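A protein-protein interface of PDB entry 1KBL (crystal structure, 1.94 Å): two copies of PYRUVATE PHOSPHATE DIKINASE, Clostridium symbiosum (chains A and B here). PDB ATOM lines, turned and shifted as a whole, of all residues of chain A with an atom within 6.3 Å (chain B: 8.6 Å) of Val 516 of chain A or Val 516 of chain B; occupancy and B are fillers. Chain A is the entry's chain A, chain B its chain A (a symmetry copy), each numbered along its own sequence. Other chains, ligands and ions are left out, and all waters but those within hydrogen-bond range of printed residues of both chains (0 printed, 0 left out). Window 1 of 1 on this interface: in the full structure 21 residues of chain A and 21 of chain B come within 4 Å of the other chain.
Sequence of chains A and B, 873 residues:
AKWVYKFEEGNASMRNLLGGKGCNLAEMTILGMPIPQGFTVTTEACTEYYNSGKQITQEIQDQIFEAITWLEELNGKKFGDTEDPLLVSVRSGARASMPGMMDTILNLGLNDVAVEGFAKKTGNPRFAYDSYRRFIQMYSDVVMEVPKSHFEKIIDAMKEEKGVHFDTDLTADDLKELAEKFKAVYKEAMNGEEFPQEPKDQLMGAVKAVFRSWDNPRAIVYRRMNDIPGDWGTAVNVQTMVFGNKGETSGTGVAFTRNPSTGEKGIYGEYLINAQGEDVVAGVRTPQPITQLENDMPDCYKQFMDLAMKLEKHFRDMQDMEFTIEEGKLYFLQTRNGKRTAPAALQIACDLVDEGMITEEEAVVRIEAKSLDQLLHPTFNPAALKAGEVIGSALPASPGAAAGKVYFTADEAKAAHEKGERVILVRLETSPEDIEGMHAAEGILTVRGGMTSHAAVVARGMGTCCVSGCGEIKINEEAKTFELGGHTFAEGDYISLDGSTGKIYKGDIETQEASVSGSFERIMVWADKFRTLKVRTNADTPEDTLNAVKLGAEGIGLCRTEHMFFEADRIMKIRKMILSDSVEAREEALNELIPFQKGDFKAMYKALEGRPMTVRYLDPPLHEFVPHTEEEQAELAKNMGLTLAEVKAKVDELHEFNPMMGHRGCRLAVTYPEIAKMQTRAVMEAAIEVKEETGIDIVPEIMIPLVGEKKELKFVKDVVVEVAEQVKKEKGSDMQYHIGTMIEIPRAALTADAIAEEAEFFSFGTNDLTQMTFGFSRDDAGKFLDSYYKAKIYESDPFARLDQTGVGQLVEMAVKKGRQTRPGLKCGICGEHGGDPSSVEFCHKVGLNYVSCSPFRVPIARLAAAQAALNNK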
ATOM      1  N   LEU A 375     -10.183 -30.395  29.878  1.00  0.00           N
ATOM      2  CA  LEU A 375     -10.245 -30.438  28.412  1.00  0.00           C
ATOM      3  C   LEU A 375      -9.322 -31.451  27.785  1.00  0.00           C
ATOM      4  O   LEU A 375      -9.513 -31.810  26.640  1.00  0.00           O
ATOM      5  CB  LEU A 375      -9.870 -29.067  27.796  1.00  0.00           C
ATOM      6  CG  LEU A 375     -10.610 -27.859  28.345  1.00  0.00           C
ATOM      7  CD1 LEU A 375     -10.048 -26.514  27.742  1.00  0.00           C
ATOM      8  CD2 LEU A 375     -12.082 -28.050  28.063  1.00  0.00           C
ATOM      9  N   LEU A 376      -8.277 -31.830  28.504  1.00  0.00           N
ATOM     10  CA  LEU A 376      -7.289 -32.754  27.972  1.00  0.00           C
ATOM     11  C   LEU A 376      -7.331 -34.158  28.539  1.00  0.00           C
ATOM     12  O   LEU A 376      -6.423 -34.954  28.322  1.00  0.00           O
ATOM     13  CB  LEU A 376      -5.876 -32.171  28.130  1.00  0.00           C
ATOM     14  CG  LEU A 376      -5.691 -30.875  27.304  1.00  0.00           C
ATOM     15  CD1 LEU A 376      -4.285 -30.411  27.466  1.00  0.00           C
ATOM     16  CD2 LEU A 376      -5.986 -31.090  25.815  1.00  0.00           C
ATOM     17  N   ALA A 514      -7.878 -36.497  23.800  1.00  0.00           N
ATOM     18  CA  ALA A 514      -8.975 -35.619  23.445  1.00  0.00           C
ATOM     19  C   ALA A 514      -8.550 -34.650  22.382  1.00  0.00           C
ATOM     20  O   ALA A 514      -7.383 -34.620  22.019  1.00  0.00           O
ATOM     21  CB  ALA A 514      -9.414 -34.849  24.674  1.00  0.00           C
ATOM     22  N   SER A 515      -9.506 -33.852  21.911  1.00  0.00           N
ATOM     23  CA  SER A 515      -9.288 -32.793  20.913  1.00  0.00           C
ATOM     24  C   SER A 515      -9.593 -31.418  21.591  1.00  0.00           C
ATOM     25  O   SER A 515      -9.144 -31.202  22.718  1.00  0.00           O
ATOM     26  CB  SER A 515     -10.226 -33.019  19.746  1.00  0.00           C
ATOM     27  OG  SER A 515     -11.559 -33.090  20.239  1.00  0.00           O
ATOM     28  N   VAL A 516     -10.332 -30.501  20.932  1.00  0.00           N
ATOM     29  CA  VAL A 516     -10.676 -29.167  21.511  1.00  0.00           C
ATOM     30  C   VAL A 516     -11.851 -28.358  20.898  1.00  0.00           C
ATOM     31  O   VAL A 516     -12.004 -28.221  19.698  1.00  0.00           O
ATOM     32  CB  VAL A 516      -9.440 -28.211  21.586  1.00  0.00           C
ATOM     33  CG1 VAL A 516      -8.769 -28.333  22.946  1.00  0.00           C
ATOM     34  CG2 VAL A 516      -8.402 -28.538  20.486  1.00  0.00           C
ATOM     35  N   SER A 517     -12.690 -27.792  21.746  1.00  0.00           N
ATOM     36  CA  SER A 517     -13.828 -27.022  21.255  1.00  0.00           C
ATOM     37  C   SER A 517     -13.399 -25.803  20.455  1.00  0.00           C
ATOM     38  O   SER A 517     -12.226 -25.611  20.168  1.00  0.00           O
ATOM     39  CB  SER A 517     -14.705 -26.564  22.424  1.00  0.00           C
ATOM     40  OG  SER A 517     -14.079 -25.553  23.202  1.00  0.00           O
ATOM     41  N   GLY A 518     -14.381 -24.978  20.117  1.00  0.00           N
ATOM     42  CA  GLY A 518     -14.139 -23.756  19.364  1.00  0.00           C
ATOM     43  C   GLY A 518     -14.371 -22.612  20.324  1.00  0.00           C
ATOM     44  O   GLY A 518     -13.929 -21.440  20.109  1.00  0.00           O
ATOM     45  N   PHE A 520     -13.241 -23.110  23.098  1.00  0.00           N
ATOM     46  CA  PHE A 520     -11.938 -23.137  23.735  1.00  0.00           C
ATOM     47  C   PHE A 520     -10.973 -22.312  22.879  1.00  0.00           C
ATOM     48  O   PHE A 520     -10.197 -21.514  23.407  1.00  0.00           O
ATOM     49  CB  PHE A 520     -11.352 -24.559  23.852  1.00  0.00           C
ATOM     50  CG  PHE A 520      -9.864 -24.551  24.077  1.00  0.00           C
ATOM     51  CD1 PHE A 520      -9.323 -24.358  25.368  1.00  0.00           C
ATOM     52  CD2 PHE A 520      -8.992 -24.605  23.006  1.00  0.00           C
ATOM     53  CE1 PHE A 520      -7.939 -24.207  25.575  1.00  0.00           C
ATOM     54  CE2 PHE A 520      -7.578 -24.456  23.201  1.00  0.00           C
ATOM     55  CZ  PHE A 520      -7.055 -24.254  24.495  1.00  0.00           C
ATOM     56  N   GLU A 521     -11.012 -22.503  21.561  1.00  0.00           N
ATOM     57  CA  GLU A 521     -10.083 -21.757  20.725  1.00  0.00           C
ATOM     58  C   GLU A 521     -10.468 -20.316  20.801  1.00  0.00           C
ATOM     59  O   GLU A 521      -9.602 -19.462  20.764  1.00  0.00           O
ATOM     60  CB  GLU A 521     -10.122 -22.242  19.281  1.00  0.00           C
ATOM     61  CG  GLU A 521      -9.783 -23.737  19.186  1.00  0.00           C
ATOM     62  CD  GLU A 521      -8.302 -24.027  19.130  1.00  0.00           C
ATOM     63  OE1 GLU A 521      -7.553 -23.473  19.958  1.00  0.00           O
ATOM     64  OE2 GLU A 521      -7.889 -24.810  18.251  1.00  0.00           O
ATOM     65  N   LYS A 550       0.579 -27.123  19.406  1.00  0.00           N
ATOM     66  CA  LYS A 550      -0.801 -27.199  19.000  1.00  0.00           C
ATOM     67  C   LYS A 550      -1.705 -26.573  20.060  1.00  0.00           C
ATOM     68  O   LYS A 550      -2.764 -26.059  19.711  1.00  0.00           O
ATOM     69  CB  LYS A 550      -1.231 -28.632  18.731  1.00  0.00           C
ATOM     70  CG  LYS A 550      -2.677 -28.689  18.204  1.00  0.00           C
ATOM     71  CD  LYS A 550      -3.192 -30.112  18.012  1.00  0.00           C
ATOM     72  CE  LYS A 550      -2.324 -30.881  17.038  1.00  0.00           C
ATOM     73  NZ  LYS A 550      -0.940 -31.050  17.561  1.00  0.00           N
ATOM     74  N   LEU A 551      -1.289 -26.588  21.333  1.00  0.00           N
ATOM     75  CA  LEU A 551      -2.121 -25.980  22.391  1.00  0.00           C
ATOM     76  C   LEU A 551      -1.798 -24.497  22.625  1.00  0.00           C
ATOM     77  O   LEU A 551      -2.429 -23.826  23.446  1.00  0.00           O
ATOM     78  CB  LEU A 551      -1.987 -26.754  23.665  1.00  0.00           C
ATOM     79  CG  LEU A 551      -2.592 -28.150  23.451  1.00  0.00           C
ATOM     80  CD1 LEU A 551      -2.317 -29.069  24.590  1.00  0.00           C
ATOM     81  CD2 LEU A 551      -4.102 -27.994  23.207  1.00  0.00           C
ATOM     82  N   LEU B 346     -10.310 -21.327   7.239  1.00  0.00           N
ATOM     83  CA  LEU B 346     -10.893 -20.904   8.521  1.00  0.00           C
ATOM     84  C   LEU B 346      -9.798 -20.171   9.351  1.00  0.00           C
ATOM     85  O   LEU B 346      -9.973 -19.022   9.840  1.00  0.00           O
ATOM     86  CB  LEU B 346     -11.398 -22.162   9.257  1.00  0.00           C
ATOM     87  CG  LEU B 346     -12.438 -22.982   8.462  1.00  0.00           C
ATOM     88  CD1 LEU B 346     -12.787 -24.216   9.178  1.00  0.00           C
ATOM     89  CD2 LEU B 346     -13.669 -22.161   8.247  1.00  0.00           C
ATOM     90  N   LEU B 372     -16.007 -27.272   3.048  1.00  0.00           N
ATOM     91  CA  LEU B 372     -16.086 -27.709   4.456  1.00  0.00           C
ATOM     92  C   LEU B 372     -16.397 -29.201   4.640  1.00  0.00           C
ATOM     93  O   LEU B 372     -16.391 -29.697   5.742  1.00  0.00           O
ATOM     94  CB  LEU B 372     -17.073 -26.886   5.294  1.00  0.00           C
ATOM     95  CG  LEU B 372     -16.874 -25.372   5.310  1.00  0.00           C
ATOM     96  CD1 LEU B 372     -17.821 -24.716   6.246  1.00  0.00           C
ATOM     97  CD2 LEU B 372     -15.517 -25.065   5.718  1.00  0.00           C
ATOM     98  N   GLN B 374     -14.442 -31.286   3.797  1.00  0.00           N
ATOM     99  CA  GLN B 374     -13.128 -31.765   4.222  1.00  0.00           C
ATOM    100  C   GLN B 374     -13.017 -31.900   5.765  1.00  0.00           C
ATOM    101  O   GLN B 374     -12.358 -32.798   6.297  1.00  0.00           O
ATOM    102  CB  GLN B 374     -12.059 -30.789   3.731  1.00  0.00           C
ATOM    103  CG  GLN B 374     -11.863 -30.711   2.183  1.00  0.00           C
ATOM    104  CD  GLN B 374     -10.877 -29.587   1.857  1.00  0.00           C
ATOM    105  OE1 GLN B 374      -9.891 -29.385   2.593  1.00  0.00           O
ATOM    106  NE2 GLN B 374     -11.137 -28.839   0.783  1.00  0.00           N
ATOM    107  N   LEU B 375     -13.641 -30.987   6.492  1.00  0.00           N
ATOM    108  CA  LEU B 375     -13.568 -31.008   7.958  1.00  0.00           C
ATOM    109  C   LEU B 375     -14.095 -32.273   8.584  1.00  0.00           C
ATOM    110  O   LEU B 375     -13.794 -32.548   9.729  1.00  0.00           O
ATOM    111  CB  LEU B 375     -14.384 -29.844   8.575  1.00  0.00           C
ATOM    112  CG  LEU B 375     -14.094 -28.456   8.027  1.00  0.00           C
ATOM    113  CD1 LEU B 375     -15.078 -27.381   8.631  1.00  0.00           C
ATOM    114  CD2 LEU B 375     -12.644 -28.141   8.309  1.00  0.00           C
ATOM    115  N   LEU B 376     -14.951 -32.982   7.864  1.00  0.00           N
ATOM    116  CA  LEU B 376     -15.570 -34.186   8.396  1.00  0.00           C
ATOM    117  C   LEU B 376     -15.056 -35.493   7.828  1.00  0.00           C
ATOM    118  O   LEU B 376     -15.643 -36.548   8.045  1.00  0.00           O
ATOM    119  CB  LEU B 376     -17.096 -34.113   8.238  1.00  0.00           C
ATOM    120  CG  LEU B 376     -17.707 -32.956   9.065  1.00  0.00           C
ATOM    121  CD1 LEU B 376     -19.188 -32.994   8.904  1.00  0.00           C
ATOM    122  CD2 LEU B 376     -17.357 -33.060  10.554  1.00  0.00           C
ATOM    123  N   THR B 379     -10.388 -39.225  10.218  1.00  0.00           N
ATOM    124  CA  THR B 379      -8.936 -39.073  10.412  1.00  0.00           C
ATOM    125  C   THR B 379      -8.493 -40.458  10.931  1.00  0.00           C
ATOM    126  O   THR B 379      -9.344 -41.251  11.298  1.00  0.00           O
ATOM    127  CB  THR B 379      -8.612 -37.992  11.444  1.00  0.00           C
ATOM    128  OG1 THR B 379      -9.207 -38.345  12.697  1.00  0.00           O
ATOM    129  CG2 THR B 379      -9.134 -36.581  10.969  1.00  0.00           C
ATOM    130  N   GLU B 513     -14.053 -41.027  13.178  1.00  0.00           N
ATOM    131  CA  GLU B 513     -14.641 -39.743  12.827  1.00  0.00           C
ATOM    132  C   GLU B 513     -13.851 -38.555  13.377  1.00  0.00           C
ATOM    133  O   GLU B 513     -13.342 -38.579  14.486  1.00  0.00           O
ATOM    134  CB  GLU B 513     -16.097 -39.674  13.281  1.00  0.00           C
ATOM    135  CG  GLU B 513     -17.034 -39.083  12.205  1.00  0.00           C
ATOM    136  CD  GLU B 513     -16.660 -37.643  11.751  1.00  0.00           C
ATOM    137  OE1 GLU B 513     -16.022 -37.456  10.624  1.00  0.00           O
ATOM    138  OE2 GLU B 513     -17.034 -36.732  12.565  1.00  0.00           O
ATOM    139  N   ALA B 514     -13.752 -37.513  12.565  1.00  0.00           N
ATOM    140  CA  ALA B 514     -13.015 -36.318  12.921  1.00  0.00           C
ATOM    141  C   ALA B 514     -13.742 -35.549  13.985  1.00  0.00           C
ATOM    142  O   ALA B 514     -14.850 -35.914  14.347  1.00  0.00           O
ATOM    143  CB  ALA B 514     -12.863 -35.443  11.693  1.00  0.00           C
ATOM    144  N   SER B 515     -13.111 -34.475  14.456  1.00  0.00           N
ATOM    145  CA  SER B 515     -13.673 -33.553  15.455  1.00  0.00           C
ATOM    146  C   SER B 515     -13.850 -32.155  14.778  1.00  0.00           C
ATOM    147  O   SER B 515     -14.346 -32.102  13.651  1.00  0.00           O
ATOM    148  CB  SER B 515     -12.714 -33.450  16.623  1.00  0.00           C
ATOM    149  OG  SER B 515     -11.436 -33.067  16.129  1.00  0.00           O
ATOM    150  N   VAL B 516     -13.464 -31.043  15.438  1.00  0.00           N
ATOM    151  CA  VAL B 516     -13.590 -29.671  14.860  1.00  0.00           C
ATOM    152  C   VAL B 516     -12.757 -28.513  15.474  1.00  0.00           C
ATOM    153  O   VAL B 516     -12.659 -28.334  16.674  1.00  0.00           O
ATOM    154  CB  VAL B 516     -15.077 -29.188  14.786  1.00  0.00           C
ATOM    155  CG1 VAL B 516     -15.667 -29.529  13.425  1.00  0.00           C
ATOM    156  CG2 VAL B 516     -15.944 -29.846  15.885  1.00  0.00           C
ATOM    157  N   SER B 517     -12.158 -27.697  14.626  1.00  0.00           N
ATOM    158  CA  SER B 517     -11.347 -26.589  15.118  1.00  0.00           C
ATOM    159  C   SER B 517     -12.161 -25.586  15.919  1.00  0.00           C
ATOM    160  O   SER B 517     -13.331 -25.802  16.205  1.00  0.00           O
ATOM    161  CB  SER B 517     -10.675 -25.861  13.949  1.00  0.00           C
ATOM    162  OG  SER B 517     -11.606 -25.120  13.173  1.00  0.00           O
ATOM    163  N   GLY B 518     -11.516 -24.478  16.257  1.00  0.00           N
ATOM    164  CA  GLY B 518     -12.155 -23.410  17.012  1.00  0.00           C
ATOM    165  C   GLY B 518     -12.323 -22.255  16.052  1.00  0.00           C
ATOM    166  O   GLY B 518     -13.135 -21.301  16.268  1.00  0.00           O
ATOM    167  N   SER B 519     -11.508 -22.323  14.987  1.00  0.00           N
ATOM    168  CA  SER B 519     -11.639 -21.341  13.944  1.00  0.00           C
ATOM    169  C   SER B 519     -12.904 -21.811  13.214  1.00  0.00           C
ATOM    170  O   SER B 519     -13.592 -21.005  12.642  1.00  0.00           O
ATOM    171  CB  SER B 519     -10.430 -21.304  12.997  1.00  0.00           C
ATOM    172  OG  SER B 519      -9.754 -20.067  13.149  1.00  0.00           O
ATOM    173  N   PHE B 520     -13.220 -23.103  13.278  1.00  0.00           N
ATOM    174  CA  PHE B 520     -14.437 -23.568  12.641  1.00  0.00           C
ATOM    175  C   PHE B 520     -15.623 -23.116  13.497  1.00  0.00           C
ATOM    176  O   PHE B 520     -16.623 -22.627  12.969  1.00  0.00           O
ATOM    177  CB  PHE B 520     -14.509 -25.104  12.523  1.00  0.00           C
ATOM    178  CG  PHE B 520     -15.912 -25.598  12.297  1.00  0.00           C
ATOM    179  CD1 PHE B 520     -16.487 -25.597  11.007  1.00  0.00           C
ATOM    180  CD2 PHE B 520     -16.715 -25.943  13.368  1.00  0.00           C
ATOM    181  CE1 PHE B 520     -17.841 -25.922  10.800  1.00  0.00           C
ATOM    182  CE2 PHE B 520     -18.096 -26.280  13.173  1.00  0.00           C
ATOM    183  CZ  PHE B 520     -18.657 -26.266  11.879  1.00  0.00           C
ATOM    184  N   GLU B 521     -15.522 -23.284  14.815  1.00  0.00           N
ATOM    185  CA  GLU B 521     -16.648 -22.895  15.652  1.00  0.00           C
ATOM    186  C   GLU B 521     -16.772 -21.410  15.576  1.00  0.00           C
ATOM    187  O   GLU B 521     -17.875 -20.898  15.614  1.00  0.00           O
ATOM    188  CB  GLU B 521     -16.448 -23.340  17.095  1.00  0.00           C
ATOM    189  CG  GLU B 521     -16.262 -24.862  17.189  1.00  0.00           C
ATOM    190  CD  GLU B 521     -17.559 -25.635  17.245  1.00  0.00           C
ATOM    191  OE1 GLU B 521     -18.451 -25.366  16.417  1.00  0.00           O
ATOM    192  OE2 GLU B 521     -17.684 -26.512  18.123  1.00  0.00           O
ATOM    193  N   ARG B 522     -15.651 -20.728  15.367  1.00  0.00           N
ATOM    194  CA  ARG B 522     -15.665 -19.251  15.325  1.00  0.00           C
ATOM    195  C   ARG B 522     -16.320 -18.755  14.066  1.00  0.00           C
ATOM    196  O   ARG B 522     -17.067 -17.744  14.066  1.00  0.00           O
ATOM    197  CB  ARG B 522     -14.220 -18.649  15.371  1.00  0.00           C
ATOM    198  CG  ARG B 522     -13.651 -18.377  16.728  1.00  0.00           C
ATOM    199  CD  ARG B 522     -12.319 -17.635  16.627  1.00  0.00           C
ATOM    200  NE  ARG B 522     -12.459 -16.163  16.682  1.00  0.00           N
ATOM    201  CZ  ARG B 522     -11.497 -15.333  16.293  1.00  0.00           C
ATOM    202  NH1 ARG B 522     -10.351 -15.846  15.815  1.00  0.00           N
ATOM    203  NH2 ARG B 522     -11.655 -14.012  16.404  1.00  0.00           N
ATOM    204  N   MET B 524     -18.535 -20.373  12.279  1.00  0.00           N
ATOM    205  CA  MET B 524     -19.982 -20.656  12.438  1.00  0.00           C
ATOM    206  C   MET B 524     -20.661 -19.586  13.305  1.00  0.00           C
ATOM    207  O   MET B 524     -21.794 -19.216  13.051  1.00  0.00           O
ATOM    208  CB  MET B 524     -20.212 -21.998  13.133  1.00  0.00           C
ATOM    209  CG  MET B 524     -19.771 -23.176  12.258  1.00  0.00           C
ATOM    210  SD  MET B 524     -20.784 -23.263  10.724  1.00  0.00           S
ATOM    211  CE  MET B 524     -19.590 -23.153   9.504  1.00  0.00           C
ATOM    212  N   LYS B 550     -24.874 -31.545  16.965  1.00  0.00           N
ATOM    213  CA  LYS B 550     -23.550 -31.152  17.371  1.00  0.00           C
ATOM    214  C   LYS B 550     -22.910 -30.256  16.312  1.00  0.00           C
ATOM    215  O   LYS B 550     -22.087 -29.415  16.661  1.00  0.00           O
ATOM    216  CB  LYS B 550     -22.662 -32.355  17.640  1.00  0.00           C
ATOM    217  CG  LYS B 550     -21.281 -31.922  18.167  1.00  0.00           C
ATOM    218  CD  LYS B 550     -20.316 -33.088  18.357  1.00  0.00           C
ATOM    219  CE  LYS B 550     -20.874 -34.106  19.331  1.00  0.00           C
ATOM    220  NZ  LYS B 550     -22.120 -34.731  18.807  1.00  0.00           N
ATOM    221  N   LEU B 551     -23.297 -30.409  15.038  1.00  0.00           N
ATOM    222  CA  LEU B 551     -22.719 -29.557  13.982  1.00  0.00           C
ATOM    223  C   LEU B 551     -23.524 -28.269  13.748  1.00  0.00           C
ATOM    224  O   LEU B 551     -23.156 -27.423  12.927  1.00  0.00           O
ATOM    225  CB  LEU B 551     -22.585 -30.329  12.707  1.00  0.00           C
ATOM    226  CG  LEU B 551     -21.544 -31.440  12.920  1.00  0.00           C
ATOM    227  CD1 LEU B 551     -21.493 -32.397  11.780  1.00  0.00           C
ATOM    228  CD2 LEU B 551     -20.175 -30.783  13.164  1.00  0.00           C
ATOM    229  N   PRO B 859     -22.538 -28.095   8.343  1.00  0.00           N
ATOM    230  CA  PRO B 859     -21.609 -26.952   8.366  1.00  0.00           C
ATOM    231  C   PRO B 859     -21.645 -26.218   6.997  1.00  0.00           C
ATOM    232  O   PRO B 859     -21.686 -24.957   6.908  1.00  0.00           O
ATOM    233  CB  PRO B 859     -20.255 -27.625   8.663  1.00  0.00           C
ATOM    234  CG  PRO B 859     -20.631 -28.831   9.454  1.00  0.00           C
ATOM    235  CD  PRO B 859     -21.838 -29.360   8.671  1.00  0.00           C
ATOM    236  N   ARG B 862     -24.884 -24.261   6.787  1.00  0.00           N
ATOM    237  CA  ARG B 862     -24.868 -23.120   7.667  1.00  0.00           C
ATOM    238  C   ARG B 862     -24.039 -22.000   7.032  1.00  0.00           C
ATOM    239  O   ARG B 862     -24.472 -20.845   7.030  1.00  0.00           O
ATOM    240  CB  ARG B 862     -24.305 -23.510   9.040  1.00  0.00           C
ATOM    241  CG  ARG B 862     -25.309 -24.242   9.975  1.00  0.00           C
ATOM    242  CD  ARG B 862     -24.666 -24.609  11.353  1.00  0.00           C
ATOM    243  NE  ARG B 862     -24.390 -23.524  12.308  1.00  0.00           N
ATOM    244  CZ  ARG B 862     -23.499 -23.666  13.282  1.00  0.00           C
ATOM    245  NH1 ARG B 862     -22.820 -24.799  13.367  1.00  0.00           N
ATOM    246  NH2 ARG B 862     -23.355 -22.746  14.214  1.00  0.00           N
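The backbone carbonyl oxygen of Val 516 of chain A lies close to the backbone carbonyl oxygen of Val 516 of chain B.
The side-chain hydroxyl (OG) of Ser 517 of chain B is in hydrogen-bond range of the backbone NH (N) of Phe 520 of chain B (2.6 Å).
The side-chain hydroxyl of Ser 517 of chain A is in hydrogen-bond range of the backbone NH of Phe 520 of chain A, 2.6 Å away.
The backbone NH (N) of Ser 519 of chain B sits at hydrogen-bond distance from the side-chain hydroxyl (OG) of Ser 517 of chain B (3.3 Å).
CB of Ser 515 of chain B touches OG of Ser 515 of chain A, at 3.8 Å.
Ser 517 of chain A touches Gly 518 of chain B (O to CA, 3.8 Å).
O of Ser 517 of chain B touches CA of Gly 518 of chain A, at 3.8 Å.
Gly 518 of chain A touches Gly 518 of chain B.
CA of Gly 518 of chain A touches CG of Glu 521 of chain B (3.2 Å).
Gly 518 of chain B touches Glu 521 of chain A.
Val 516 of chain A touches just one residue of chain B: Val 516.
Of the printed residues of chain B, Glu 521 of chain A touches Gly 518 (3.2 Å).
Of chain A, only Val 516 (3.1 Å) comes within 4 Å of Val 516 of chain B.
Of the printed residues of chain A, Ser 517 of chain B touches Gly 518.
Of the printed residues of chain A, Glu 521 of chain B touches Gly 518.
The nearest residue of chain B that does not touch Val 516 of chain A is Ser 517 of chain B (4.5 Å).
The nearest printed residue of chain A that does not touch Ser 517 of chain B is Ser 517 of chain A (4.1 Å).
Printed residues of chain A that touch a printed residue of chain B: Ser 515, Val 516, Ser 517, Gly 518 and Glu 521.
Of the 21 printed residues of chain B, 5 touch a printed residue of chain A.
Among the printed residues, no Asp or Glu carboxylate lies within 4 Å of a Lys or Arg side-chain nitrogen of the other chain.
Ser 515 of chain A touches its own counterpart, Ser 515 of chain B.
Ser 517 of chain A touches Gly 518 of chain B, and with the chains exchanged Gly 518 of chain A touches Ser 517 of chain B.
Gly 518 of chain A touches its own counterpart, Gly 518 of chain B.
Gly 518 of chain A touches Glu 521 of chain B, and with the chains exchanged Glu 521 of chain A touches Gly 518 of chain B.
11 positions are printed for both chains.
Of the 7 pairs that touch across the chains among the printed residues, 7 have their exchanged pair printed and touching as well.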
